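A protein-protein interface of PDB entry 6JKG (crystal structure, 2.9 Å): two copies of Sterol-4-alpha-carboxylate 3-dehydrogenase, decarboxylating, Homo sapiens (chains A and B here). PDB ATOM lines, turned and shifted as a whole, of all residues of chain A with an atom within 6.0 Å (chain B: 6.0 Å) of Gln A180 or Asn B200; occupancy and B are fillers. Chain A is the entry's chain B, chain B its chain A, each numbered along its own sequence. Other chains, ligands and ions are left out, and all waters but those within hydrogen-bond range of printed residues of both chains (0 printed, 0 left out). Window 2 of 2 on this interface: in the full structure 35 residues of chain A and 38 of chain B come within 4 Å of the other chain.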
ATOM      1  N   PRO A 179     -17.965 -10.744  20.085  1.00  0.00           N
ATOM      2  CA  PRO A 179     -18.018 -11.290  21.445  1.00  0.00           C
ATOM      3  C   PRO A 179     -17.161 -12.554  21.583  1.00  0.00           C
ATOM      4  O   PRO A 179     -15.953 -12.440  21.669  1.00  0.00           O
ATOM      5  CB  PRO A 179     -19.497 -11.628  21.692  1.00  0.00           C
ATOM      6  CG  PRO A 179     -20.031 -11.970  20.328  1.00  0.00           C
ATOM      7  CD  PRO A 179     -19.327 -10.999  19.408  1.00  0.00           C
ATOM      8  N   GLN A 180     -17.808 -13.721  21.613  1.00  0.00           N
ATOM      9  CA  GLN A 180     -17.039 -14.982  21.742  1.00  0.00           C
ATOM     10  C   GLN A 180     -16.861 -15.620  20.366  1.00  0.00           C
ATOM     11  O   GLN A 180     -16.370 -16.743  20.316  1.00  0.00           O
ATOM     12  CB  GLN A 180     -17.668 -15.940  22.752  1.00  0.00           C
ATOM     13  CG  GLN A 180     -16.800 -17.166  22.990  1.00  0.00           C
ATOM     14  CD  GLN A 180     -17.281 -18.071  24.097  1.00  0.00           C
ATOM     15  OE1 GLN A 180     -18.243 -17.755  24.792  1.00  0.00           O
ATOM     16  NE2 GLN A 180     -16.632 -19.212  24.255  1.00  0.00           N
ATOM     17  N   LEU A 181     -17.264 -14.936  19.298  1.00  0.00           N
ATOM     18  CA  LEU A 181     -17.045 -15.489  17.941  1.00  0.00           C
ATOM     19  C   LEU A 181     -16.418 -14.384  17.109  1.00  0.00           C
ATOM     20  O   LEU A 181     -17.021 -13.335  16.987  1.00  0.00           O
ATOM     21  CB  LEU A 181     -18.363 -15.957  17.330  1.00  0.00           C
ATOM     22  CG  LEU A 181     -18.259 -17.250  16.529  1.00  0.00           C
ATOM     23  CD1 LEU A 181     -17.439 -18.271  17.291  1.00  0.00           C
ATOM     24  CD2 LEU A 181     -19.633 -17.807  16.212  1.00  0.00           C
ATOM     25  N   VAL A 182     -15.246 -14.654  16.557  1.00  0.00           N
ATOM     26  CA  VAL A 182     -14.485 -13.653  15.810  1.00  0.00           C
ATOM     27  C   VAL A 182     -13.862 -14.236  14.544  1.00  0.00           C
ATOM     28  O   VAL A 182     -13.333 -15.357  14.563  1.00  0.00           O
ATOM     29  CB  VAL A 182     -13.410 -13.013  16.708  1.00  0.00           C
ATOM     30  CG1 VAL A 182     -12.570 -14.084  17.363  1.00  0.00           C
ATOM     31  CG2 VAL A 182     -12.522 -12.063  15.906  1.00  0.00           C
ATOM     32  N   ILE A 184     -10.923 -14.881  12.132  1.00  0.00           N
ATOM     33  CA  ILE A 184      -9.465 -14.899  12.229  1.00  0.00           C
ATOM     34  C   ILE A 184      -8.800 -14.558  10.901  1.00  0.00           C
ATOM     35  O   ILE A 184      -7.781 -13.871  10.877  1.00  0.00           O
ATOM     36  CB  ILE A 184      -8.967 -16.260  12.753  1.00  0.00           C
ATOM     37  CG1 ILE A 184      -9.792 -16.727  13.942  1.00  0.00           C
ATOM     38  CG2 ILE A 184      -7.506 -16.188  13.147  1.00  0.00           C
ATOM     39  CD1 ILE A 184      -9.482 -18.136  14.310  1.00  0.00           C
ATOM     40  N   ILE B 198     -13.783 -18.689  11.269  1.00  0.00           N
ATOM     41  CA  ILE B 198     -14.190 -18.294  12.609  1.00  0.00           C
ATOM     42  C   ILE B 198     -13.323 -18.979  13.656  1.00  0.00           C
ATOM     43  O   ILE B 198     -12.971 -20.157  13.535  1.00  0.00           O
ATOM     44  CB  ILE B 198     -15.676 -18.627  12.831  1.00  0.00           C
ATOM     45  CG1 ILE B 198     -16.562 -17.792  11.916  1.00  0.00           C
ATOM     46  CG2 ILE B 198     -16.050 -18.396  14.265  1.00  0.00           C
ATOM     47  CD1 ILE B 198     -18.031 -18.135  12.058  1.00  0.00           C
ATOM     48  N   GLY B 199     -12.992 -18.233  14.710  1.00  0.00           N
ATOM     49  CA  GLY B 199     -12.397 -18.809  15.889  1.00  0.00           C
ATOM     50  C   GLY B 199     -13.231 -18.502  17.119  1.00  0.00           C
ATOM     51  O   GLY B 199     -14.210 -17.763  17.063  1.00  0.00           O
ATOM     52  N   ASN B 200     -12.823 -19.099  18.237  1.00  0.00           N
ATOM     53  CA  ASN B 200     -13.489 -18.883  19.522  1.00  0.00           C
ATOM     54  C   ASN B 200     -12.571 -17.972  20.328  1.00  0.00           C
ATOM     55  O   ASN B 200     -11.663 -18.426  21.027  1.00  0.00           O
ATOM     56  CB  ASN B 200     -13.764 -20.211  20.219  1.00  0.00           C
ATOM     57  CG  ASN B 200     -14.743 -20.084  21.373  1.00  0.00           C
ATOM     58  OD1 ASN B 200     -14.789 -19.069  22.068  1.00  0.00           O
ATOM     59  ND2 ASN B 200     -15.541 -21.123  21.577  1.00  0.00           N
ATOM     60  N   GLY B 201     -12.822 -16.665  20.231  1.00  0.00           N
ATOM     61  CA  GLY B 201     -11.842 -15.652  20.593  1.00  0.00           C
ATOM     62  C   GLY B 201     -11.681 -15.403  22.078  1.00  0.00           C
ATOM     63  O   GLY B 201     -11.378 -14.267  22.464  1.00  0.00           O
ATOM     64  N   LYS B 202     -11.857 -16.425  22.917  1.00  0.00           N
ATOM     65  CA  LYS B 202     -11.601 -16.237  24.342  1.00  0.00           C
ATOM     66  C   LYS B 202     -10.371 -17.019  24.790  1.00  0.00           C
ATOM     67  O   LYS B 202      -9.582 -16.525  25.603  1.00  0.00           O
ATOM     68  CB  LYS B 202     -12.831 -16.634  25.161  1.00  0.00           C
ATOM     69  CG  LYS B 202     -14.072 -15.762  24.939  1.00  0.00           C
ATOM     70  CD  LYS B 202     -15.273 -16.197  25.777  1.00  0.00           C
ATOM     71  CE  LYS B 202     -16.500 -15.345  25.500  1.00  0.00           C
ATOM     72  NZ  LYS B 202     -16.270 -13.921  25.875  1.00  0.00           N
ATOM     73  N   ASN B 203     -10.183 -18.234  24.269  1.00  0.00           N
ATOM     74  CA  ASN B 203      -9.016 -19.045  24.599  1.00  0.00           C
ATOM     75  C   ASN B 203      -7.724 -18.496  23.995  1.00  0.00           C
ATOM     76  O   ASN B 203      -6.630 -18.871  24.437  1.00  0.00           O
ATOM     77  CB  ASN B 203      -9.244 -20.501  24.171  1.00  0.00           C
ATOM     78  CG  ASN B 203      -9.323 -20.683  22.658  1.00  0.00           C
ATOM     79  OD1 ASN B 203      -8.848 -19.852  21.884  1.00  0.00           O
ATOM     80  ND2 ASN B 203      -9.928 -21.792  22.233  1.00  0.00           N
ATOM     81  N   LEU B 204      -7.833 -17.614  22.999  1.00  0.00           N
ATOM     82  CA  LEU B 204      -6.647 -17.086  22.338  1.00  0.00           C
ATOM     83  C   LEU B 204      -6.369 -15.621  22.669  1.00  0.00           C
ATOM     84  O   LEU B 204      -5.487 -15.022  22.039  1.00  0.00           O
ATOM     85  CB  LEU B 204      -6.779 -17.289  20.824  1.00  0.00           C
ATOM     86  CG  LEU B 204      -8.121 -16.916  20.195  1.00  0.00           C
ATOM     87  CD1 LEU B 204      -8.145 -15.457  19.739  1.00  0.00           C
ATOM     88  CD2 LEU B 204      -8.429 -17.854  19.041  1.00  0.00           C
ATOM     89  N   HIS B 215      -2.623 -21.051  15.226  1.00  0.00           N
ATOM     90  CA  HIS B 215      -4.041 -21.394  15.355  1.00  0.00           C
ATOM     91  C   HIS B 215      -4.821 -21.014  14.103  1.00  0.00           C
ATOM     92  O   HIS B 215      -5.887 -21.576  13.831  1.00  0.00           O
ATOM     93  CB  HIS B 215      -4.661 -20.730  16.587  1.00  0.00           C
ATOM     94  CG  HIS B 215      -6.004 -21.287  16.942  1.00  0.00           C
ATOM     95  ND1 HIS B 215      -6.233 -22.639  17.070  1.00  0.00           N
ATOM     96  CD2 HIS B 215      -7.187 -20.682  17.195  1.00  0.00           C
ATOM     97  CE1 HIS B 215      -7.501 -22.845  17.382  1.00  0.00           C
ATOM     98  NE2 HIS B 215      -8.101 -21.672  17.468  1.00  0.00           N
ATOM     99  N   LEU B 219      -6.952 -24.006  11.973  1.00  0.00           N
ATOM    100  CA  LEU B 219      -8.374 -23.814  11.709  1.00  0.00           C
ATOM    101  C   LEU B 219      -8.674 -23.842  10.217  1.00  0.00           C
ATOM    102  O   LEU B 219      -9.643 -24.480   9.787  1.00  0.00           O
ATOM    103  CB  LEU B 219      -8.846 -22.517  12.349  1.00  0.00           C
ATOM    104  CG  LEU B 219      -9.112 -22.795  13.829  1.00  0.00           C
ATOM    105  CD1 LEU B 219      -9.793 -21.618  14.523  1.00  0.00           C
ATOM    106  CD2 LEU B 219      -9.955 -24.063  13.941  1.00  0.00           C
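N of Gly B199 sits at hydrogen-bond distance from O of Val A182, 2.9 Å away.
The side-chain amide oxygen (OD1) of Asn B200 sits at hydrogen-bond distance from the side-chain amide nitrogen (NE2) of Gln A180 (2.9 Å).
O of Asn B200 lies close to OD1 of Asn B203 (3.3 Å).
Among the printed residues, merely in contact across the chains: Gln A180 with Lys B202 (3.0 Å), Leu A181 with Gly B199 (3.3 Å), Leu A181 with Ile B198 (3.3 Å), Ile A184 with Gly B199 (3.4 Å), Ile A184 with Leu B219 (3.5 Å), Gln A180 with Gly B201 (3.5 Å), Val A182 with Ile B198 (3.6 Å), Val A182 with Gly B201 (3.7 Å) and Ile A184 with Ile B198 (3.99 Å).
Gln A180 touches just these residues of chain B: Asn B200 (2.9 Å), Gly B201 (3.5 Å) and Lys B202 (3.0 Å).
Asn B200 touches just one residue of chain A: Gln A180.
Of the printed residues of chain A, Ile B198 touches Leu A181 (3.3 Å), Val A182 (3.6 Å) and Ile A184 (3.99 Å).
Printed residues of chain A within 4 Å of Lys B202: Gln A180 (3.0 Å).
Of the printed residues of chain A, Gly B199 touches Leu A181, Val A182 and Ile A184.
The nearest residue of chain B that does not touch Gln A180 is Gly B199 (4.04 Å).
The nearest printed residue of chain B that does not touch Ile A184 is His B215 (4.5 Å).
Of the 9 printed residues of chain B, 6 touch a printed residue of chain A.
Among the printed residues, no Asp or Glu carboxylate lies within 4 Å of a Lys or Arg side-chain nitrogen of the other chain.
No position is printed for both chains.
Of the 11 pairs that touch across the chains among the printed residues, none has its exchanged pair printed and touching as well.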
